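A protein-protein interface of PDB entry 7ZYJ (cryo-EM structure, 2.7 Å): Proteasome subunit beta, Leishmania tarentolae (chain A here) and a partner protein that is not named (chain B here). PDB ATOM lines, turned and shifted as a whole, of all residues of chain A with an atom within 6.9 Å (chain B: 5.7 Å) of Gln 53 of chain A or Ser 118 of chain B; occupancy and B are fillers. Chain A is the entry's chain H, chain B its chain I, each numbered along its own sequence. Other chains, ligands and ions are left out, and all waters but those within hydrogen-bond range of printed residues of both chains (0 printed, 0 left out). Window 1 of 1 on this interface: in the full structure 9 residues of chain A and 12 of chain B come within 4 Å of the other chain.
Among the printed residues, merely in contact across the chains: Ala 49 of chain A with Ser 118 of chain B (3.8 Å), Ala 50 of chain A with His 116 of chain B (3.3 Å), Ala 50 of chain A with Gly 117 of chain B (3.97 Å), Ala 50 of chain A with Ser 118 of chain B (3.5 Å) and Gln 53 of chain A with Ser 118 of chain B (3.6 Å).
The backbone carbonyl oxygen (O) of Ala 49 of chain A sits at hydrogen-bond distance from the side-chain hydroxyl (OG1) of Thr 52 of chain A.
Of the printed residues of chain B, Gln 53 of chain A touches Lys 84, Ser 118 and Thr 119. Ser 118 of chain B touches just these residues of chain A: Ala 49, Ala 50 and Gln 53. Gly 117 of chain B touches just one residue of chain A: Ala 50. Printed residues of chain B within 4 Å of Ala 50 of chain A: His 116 (3.3 Å), Gly 117 (3.97 Å) and Ser 118 (3.5 Å). Printed residues of chain A within 4 Å of Lys 84 of chain B: Gln 53 (2.9 Å) and Glu 57 (3.0 Å). Of the printed residues of chain A, His 116 of chain B touches Ala 50. Of the printed residues of chain A, Thr 119 of chain B touches Gln 53 (3.1 Å). Thr 52 of chain A touches none of the printed residues of chain B. Thr 112 of chain B touches none of the printed residues of chain A.
The side-chain amide oxygen of Gln 53 of chain A is in hydrogen-bond range of the backbone NH of Thr 119 of chain B (3.1 Å). NZ of Lys 84 of chain B is in hydrogen-bond range of OE1 of Gln 53 of chain A. The side-chain carboxylate of Glu 57 of chain A lies within salt-bridge range of the side-chain amino group of Lys 84 of chain B, 3.0 Å away.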
ATOM      1  N   THR A  20      22.327 -28.030   2.718  1.00  0.00           N
ATOM      2  CA  THR A  20      21.869 -27.066   1.728  1.00  0.00           C
ATOM      3  C   THR A  20      20.732 -26.268   2.350  1.00  0.00           C
ATOM      4  O   THR A  20      19.688 -26.833   2.695  1.00  0.00           O
ATOM      5  CB  THR A  20      21.409 -27.764   0.449  1.00  0.00           C
ATOM      6  OG1 THR A  20      22.351 -28.783   0.094  1.00  0.00           O
ATOM      7  CG2 THR A  20      21.300 -26.763  -0.689  1.00  0.00           C
ATOM      8  N   ASN A  32      25.707 -34.089  -0.330  1.00  0.00           N
ATOM      9  CA  ASN A  32      27.020 -34.669  -0.607  1.00  0.00           C
ATOM     10  C   ASN A  32      27.767 -33.677  -1.492  1.00  0.00           C
ATOM     11  O   ASN A  32      27.558 -33.640  -2.708  1.00  0.00           O
ATOM     12  CB  ASN A  32      26.901 -36.035  -1.270  1.00  0.00           C
ATOM     13  CG  ASN A  32      28.174 -36.850  -1.157  1.00  0.00           C
ATOM     14  OD1 ASN A  32      29.270 -36.302  -1.075  1.00  0.00           O
ATOM     15  ND2 ASN A  32      28.031 -38.169  -1.150  1.00  0.00           N
ATOM     16  N   THR A  35      32.183 -34.253  -4.821  1.00  0.00           N
ATOM     17  CA  THR A  35      31.710 -34.708  -6.118  1.00  0.00           C
ATOM     18  C   THR A  35      32.845 -35.386  -6.871  1.00  0.00           C
ATOM     19  O   THR A  35      33.932 -34.816  -7.013  1.00  0.00           O
ATOM     20  CB  THR A  35      31.157 -33.538  -6.935  1.00  0.00           C
ATOM     21  OG1 THR A  35      30.082 -32.920  -6.217  1.00  0.00           O
ATOM     22  CG2 THR A  35      30.649 -34.020  -8.279  1.00  0.00           C
ATOM     23  N   ARG A  45      32.433 -28.468  -3.466  1.00  0.00           N
ATOM     24  CA  ARG A  45      31.635 -27.416  -4.079  1.00  0.00           C
ATOM     25  C   ARG A  45      31.020 -26.538  -2.999  1.00  0.00           C
ATOM     26  O   ARG A  45      30.456 -27.050  -2.026  1.00  0.00           O
ATOM     27  CB  ARG A  45      30.532 -28.023  -4.949  1.00  0.00           C
ATOM     28  CG  ARG A  45      31.041 -28.907  -6.073  1.00  0.00           C
ATOM     29  CD  ARG A  45      29.898 -29.593  -6.807  1.00  0.00           C
ATOM     30  NE  ARG A  45      29.117 -30.457  -5.929  1.00  0.00           N
ATOM     31  CZ  ARG A  45      27.908 -30.165  -5.471  1.00  0.00           C
ATOM     32  NH1 ARG A  45      27.304 -29.030  -5.784  1.00  0.00           N
ATOM     33  NH2 ARG A  45      27.288 -31.033  -4.676  1.00  0.00           N
ATOM     34  N   SER A  48      26.362 -21.725  -5.230  1.00  0.00           N
ATOM     35  CA  SER A  48      25.144 -22.140  -5.913  1.00  0.00           C
ATOM     36  C   SER A  48      25.195 -23.631  -6.215  1.00  0.00           C
ATOM     37  O   SER A  48      26.134 -24.115  -6.853  1.00  0.00           O
ATOM     38  CB  SER A  48      24.963 -21.342  -7.201  1.00  0.00           C
ATOM     39  OG  SER A  48      23.872 -21.837  -7.958  1.00  0.00           O
ATOM     40  N   ALA A  49      24.177 -24.361  -5.753  1.00  0.00           N
ATOM     41  CA  ALA A  49      24.166 -25.808  -5.935  1.00  0.00           C
ATOM     42  C   ALA A  49      24.036 -26.184  -7.405  1.00  0.00           C
ATOM     43  O   ALA A  49      24.751 -27.067  -7.888  1.00  0.00           O
ATOM     44  CB  ALA A  49      23.032 -26.429  -5.119  1.00  0.00           C
ATOM     45  N   ALA A  50      23.131 -25.525  -8.132  1.00  0.00           N
ATOM     46  CA  ALA A  50      22.929 -25.850  -9.540  1.00  0.00           C
ATOM     47  C   ALA A  50      24.178 -25.551 -10.360  1.00  0.00           C
ATOM     48  O   ALA A  50      24.595 -26.361 -11.197  1.00  0.00           O
ATOM     49  CB  ALA A  50      21.726 -25.083 -10.087  1.00  0.00           C
ATOM     50  N   ASP A  51      24.791 -24.388 -10.128  1.00  0.00           N
ATOM     51  CA  ASP A  51      25.977 -24.006 -10.887  1.00  0.00           C
ATOM     52  C   ASP A  51      27.133 -24.962 -10.625  1.00  0.00           C
ATOM     53  O   ASP A  51      27.809 -25.408 -11.558  1.00  0.00           O
ATOM     54  CB  ASP A  51      26.375 -22.570 -10.545  1.00  0.00           C
ATOM     55  CG  ASP A  51      25.441 -21.545 -11.154  1.00  0.00           C
ATOM     56  OD1 ASP A  51      25.200 -21.613 -12.377  1.00  0.00           O
ATOM     57  OD2 ASP A  51      24.948 -20.670 -10.414  1.00  0.00           O
ATOM     58  N   THR A  52      27.371 -25.293  -9.353  1.00  0.00           N
ATOM     59  CA  THR A  52      28.469 -26.196  -9.024  1.00  0.00           C
ATOM     60  C   THR A  52      28.209 -27.599  -9.556  1.00  0.00           C
ATOM     61  O   THR A  52      29.133 -28.263 -10.041  1.00  0.00           O
ATOM     62  CB  THR A  52      28.695 -26.231  -7.513  1.00  0.00           C
ATOM     63  OG1 THR A  52      27.457 -26.500  -6.845  1.00  0.00           O
ATOM     64  CG2 THR A  52      29.256 -24.908  -7.027  1.00  0.00           C
ATOM     65  N   GLN A  53      26.961 -28.064  -9.483  1.00  0.00           N
ATOM     66  CA  GLN A  53      26.633 -29.378 -10.024  1.00  0.00           C
ATOM     67  C   GLN A  53      26.861 -29.426 -11.529  1.00  0.00           C
ATOM     68  O   GLN A  53      27.446 -30.387 -12.043  1.00  0.00           O
ATOM     69  CB  GLN A  53      25.186 -29.738  -9.690  1.00  0.00           C
ATOM     70  CG  GLN A  53      24.986 -30.254  -8.277  1.00  0.00           C
ATOM     71  CD  GLN A  53      23.535 -30.565  -7.974  1.00  0.00           C
ATOM     72  OE1 GLN A  53      22.724 -30.739  -8.881  1.00  0.00           O
ATOM     73  NE2 GLN A  53      23.200 -30.630  -6.691  1.00  0.00           N
ATOM     74  N   ALA A  54      26.416 -28.394 -12.252  1.00  0.00           N
ATOM     75  CA  ALA A  54      26.621 -28.363 -13.695  1.00  0.00           C
ATOM     76  C   ALA A  54      28.103 -28.299 -14.042  1.00  0.00           C
ATOM     77  O   ALA A  54      28.566 -28.992 -14.957  1.00  0.00           O
ATOM     78  CB  ALA A  54      25.874 -27.179 -14.306  1.00  0.00           C
ATOM     79  N   LEU A  55      28.864 -27.473 -13.316  1.00  0.00           N
ATOM     80  CA  LEU A  55      30.298 -27.372 -13.560  1.00  0.00           C
ATOM     81  C   LEU A  55      30.987 -28.712 -13.338  1.00  0.00           C
ATOM     82  O   LEU A  55      31.802 -29.145 -14.162  1.00  0.00           O
ATOM     83  CB  LEU A  55      30.901 -26.310 -12.638  1.00  0.00           C
ATOM     84  CG  LEU A  55      30.783 -24.828 -12.998  1.00  0.00           C
ATOM     85  CD1 LEU A  55      31.183 -23.987 -11.803  1.00  0.00           C
ATOM     86  CD2 LEU A  55      31.643 -24.474 -14.189  1.00  0.00           C
ATOM     87  N   ALA A  56      30.662 -29.386 -12.232  1.00  0.00           N
ATOM     88  CA  ALA A  56      31.289 -30.666 -11.929  1.00  0.00           C
ATOM     89  C   ALA A  56      30.915 -31.725 -12.954  1.00  0.00           C
ATOM     90  O   ALA A  56      31.771 -32.507 -13.379  1.00  0.00           O
ATOM     91  CB  ALA A  56      30.900 -31.118 -10.522  1.00  0.00           C
ATOM     92  N   GLU A  57      29.646 -31.772 -13.364  1.00  0.00           N
ATOM     93  CA  GLU A  57      29.234 -32.752 -14.364  1.00  0.00           C
ATOM     94  C   GLU A  57      29.932 -32.511 -15.696  1.00  0.00           C
ATOM     95  O   GLU A  57      30.400 -33.459 -16.339  1.00  0.00           O
ATOM     96  CB  GLU A  57      27.715 -32.727 -14.528  1.00  0.00           C
ATOM     97  CG  GLU A  57      26.965 -33.216 -13.298  1.00  0.00           C
ATOM     98  CD  GLU A  57      25.460 -33.164 -13.466  1.00  0.00           C
ATOM     99  OE1 GLU A  57      24.991 -32.631 -14.491  1.00  0.00           O
ATOM    100  OE2 GLU A  57      24.746 -33.661 -12.571  1.00  0.00           O
ATOM    101  N   ARG A  58      30.027 -31.248 -16.123  1.00  0.00           N
ATOM    102  CA  ARG A  58      30.714 -30.948 -17.374  1.00  0.00           C
ATOM    103  C   ARG A  58      32.192 -31.313 -17.301  1.00  0.00           C
ATOM    104  O   ARG A  58      32.743 -31.892 -18.246  1.00  0.00           O
ATOM    105  CB  ARG A  58      30.539 -29.473 -17.729  1.00  0.00           C
ATOM    106  CG  ARG A  58      31.139 -29.082 -19.069  1.00  0.00           C
ATOM    107  CD  ARG A  58      30.266 -29.535 -20.224  1.00  0.00           C
ATOM    108  NE  ARG A  58      30.713 -30.809 -20.773  1.00  0.00           N
ATOM    109  CZ  ARG A  58      30.185 -31.392 -21.840  1.00  0.00           C
ATOM    110  NH1 ARG A  58      29.178 -30.844 -22.501  1.00  0.00           N
ATOM    111  NH2 ARG A  58      30.679 -32.555 -22.254  1.00  0.00           N
ATOM    112  N   VAL A  59      32.849 -30.993 -16.184  1.00  0.00           N
ATOM    113  CA  VAL A  59      34.270 -31.301 -16.060  1.00  0.00           C
ATOM    114  C   VAL A  59      34.490 -32.808 -16.017  1.00  0.00           C
ATOM    115  O   VAL A  59      35.446 -33.325 -16.606  1.00  0.00           O
ATOM    116  CB  VAL A  59      34.868 -30.602 -14.827  1.00  0.00           C
ATOM    117  CG1 VAL A  59      36.221 -31.199 -14.486  1.00  0.00           C
ATOM    118  CG2 VAL A  59      34.992 -29.110 -15.074  1.00  0.00           C
ATOM    119  N   LYS B  84      16.980 -31.728 -15.252  1.00  0.00           N
ATOM    120  CA  LYS B  84      17.911 -30.795 -14.631  1.00  0.00           C
ATOM    121  C   LYS B  84      18.665 -29.988 -15.679  1.00  0.00           C
ATOM    122  O   LYS B  84      18.897 -28.789 -15.488  1.00  0.00           O
ATOM    123  CB  LYS B  84      18.870 -31.541 -13.699  1.00  0.00           C
ATOM    124  CG  LYS B  84      19.978 -32.326 -14.375  1.00  0.00           C
ATOM    125  CD  LYS B  84      21.031 -32.762 -13.370  1.00  0.00           C
ATOM    126  CE  LYS B  84      21.618 -31.571 -12.631  1.00  0.00           C
ATOM    127  NZ  LYS B  84      22.485 -31.991 -11.495  1.00  0.00           N
ATOM    128  N   THR B 112      14.538 -34.499  -5.876  1.00  0.00           N
ATOM    129  CA  THR B 112      13.944 -33.196  -6.137  1.00  0.00           C
ATOM    130  C   THR B 112      14.806 -32.434  -7.126  1.00  0.00           C
ATOM    131  O   THR B 112      16.037 -32.485  -7.062  1.00  0.00           O
ATOM    132  CB  THR B 112      13.791 -32.363  -4.863  1.00  0.00           C
ATOM    133  OG1 THR B 112      15.033 -32.335  -4.149  1.00  0.00           O
ATOM    134  CG2 THR B 112      12.701 -32.919  -3.988  1.00  0.00           C
ATOM    135  N   ILE B 113      14.152 -31.728  -8.040  1.00  0.00           N
ATOM    136  CA  ILE B 113      14.816 -30.842  -8.984  1.00  0.00           C
ATOM    137  C   ILE B 113      14.331 -29.431  -8.696  1.00  0.00           C
ATOM    138  O   ILE B 113      13.126 -29.152  -8.779  1.00  0.00           O
ATOM    139  CB  ILE B 113      14.536 -31.234 -10.444  1.00  0.00           C
ATOM    140  CG1 ILE B 113      14.836 -32.715 -10.675  1.00  0.00           C
ATOM    141  CG2 ILE B 113      15.379 -30.395 -11.383  1.00  0.00           C
ATOM    142  CD1 ILE B 113      13.620 -33.615 -10.592  1.00  0.00           C
ATOM    143  N   ALA B 114      15.258 -28.554  -8.343  1.00  0.00           N
ATOM    144  CA  ALA B 114      14.936 -27.163  -8.093  1.00  0.00           C
ATOM    145  C   ALA B 114      14.702 -26.433  -9.414  1.00  0.00           C
ATOM    146  O   ALA B 114      15.158 -26.885 -10.468  1.00  0.00           O
ATOM    147  CB  ALA B 114      16.062 -26.488  -7.319  1.00  0.00           C
ATOM    148  N   HIS B 116      16.173 -23.959 -10.492  1.00  0.00           N
ATOM    149  CA  HIS B 116      17.461 -23.559 -11.038  1.00  0.00           C
ATOM    150  C   HIS B 116      18.269 -24.725 -11.591  1.00  0.00           C
ATOM    151  O   HIS B 116      19.293 -24.492 -12.242  1.00  0.00           O
ATOM    152  CB  HIS B 116      18.280 -22.826  -9.971  1.00  0.00           C
ATOM    153  CG  HIS B 116      17.973 -21.365  -9.878  1.00  0.00           C
ATOM    154  ND1 HIS B 116      18.626 -20.417 -10.636  1.00  0.00           N
ATOM    155  CD2 HIS B 116      17.078 -20.689  -9.121  1.00  0.00           C
ATOM    156  CE1 HIS B 116      18.149 -19.221 -10.348  1.00  0.00           C
ATOM    157  NE2 HIS B 116      17.208 -19.358  -9.431  1.00  0.00           N
ATOM    158  N   GLY B 117      17.842 -25.964 -11.358  1.00  0.00           N
ATOM    159  CA  GLY B 117      18.487 -27.130 -11.930  1.00  0.00           C
ATOM    160  C   GLY B 117      19.205 -28.028 -10.947  1.00  0.00           C
ATOM    161  O   GLY B 117      19.675 -29.098 -11.352  1.00  0.00           O
ATOM    162  N   SER B 118      19.315 -27.642  -9.678  1.00  0.00           N
ATOM    163  CA  SER B 118      19.988 -28.480  -8.694  1.00  0.00           C
ATOM    164  C   SER B 118      19.115 -29.673  -8.328  1.00  0.00           C
ATOM    165  O   SER B 118      17.886 -29.570  -8.277  1.00  0.00           O
ATOM    166  CB  SER B 118      20.326 -27.674  -7.441  1.00  0.00           C
ATOM    167  OG  SER B 118      19.161 -27.382  -6.693  1.00  0.00           O
ATOM    168  N   THR B 119      19.756 -30.811  -8.072  1.00  0.00           N
ATOM    169  CA  THR B 119      19.059 -32.045  -7.747  1.00  0.00           C
ATOM    170  C   THR B 119      19.563 -32.617  -6.429  1.00  0.00           C
ATOM    171  O   THR B 119      20.751 -32.541  -6.106  1.00  0.00           O
ATOM    172  CB  THR B 119      19.227 -33.098  -8.853  1.00  0.00           C
ATOM    173  OG1 THR B 119      20.562 -33.619  -8.823  1.00  0.00           O
ATOM    174  CG2 THR B 119      18.951 -32.495 -10.218  1.00  0.00           C
ATOM    175  N   ASP B 120      18.637 -33.214  -5.680  1.00  0.00           N
ATOM    176  CA  ASP B 120      18.945 -33.853  -4.404  1.00  0.00           C
ATOM    177  C   ASP B 120      18.193 -35.171  -4.330  1.00  0.00           C
ATOM    178  O   ASP B 120      16.960 -35.181  -4.372  1.00  0.00           O
ATOM    179  CB  ASP B 120      18.560 -32.954  -3.225  1.00  0.00           C
ATOM    180  CG  ASP B 120      19.437 -31.723  -3.110  1.00  0.00           C
ATOM    181  OD1 ASP B 120      20.616 -31.787  -3.515  1.00  0.00           O
ATOM    182  OD2 ASP B 120      18.946 -30.688  -2.613  1.00  0.00           O
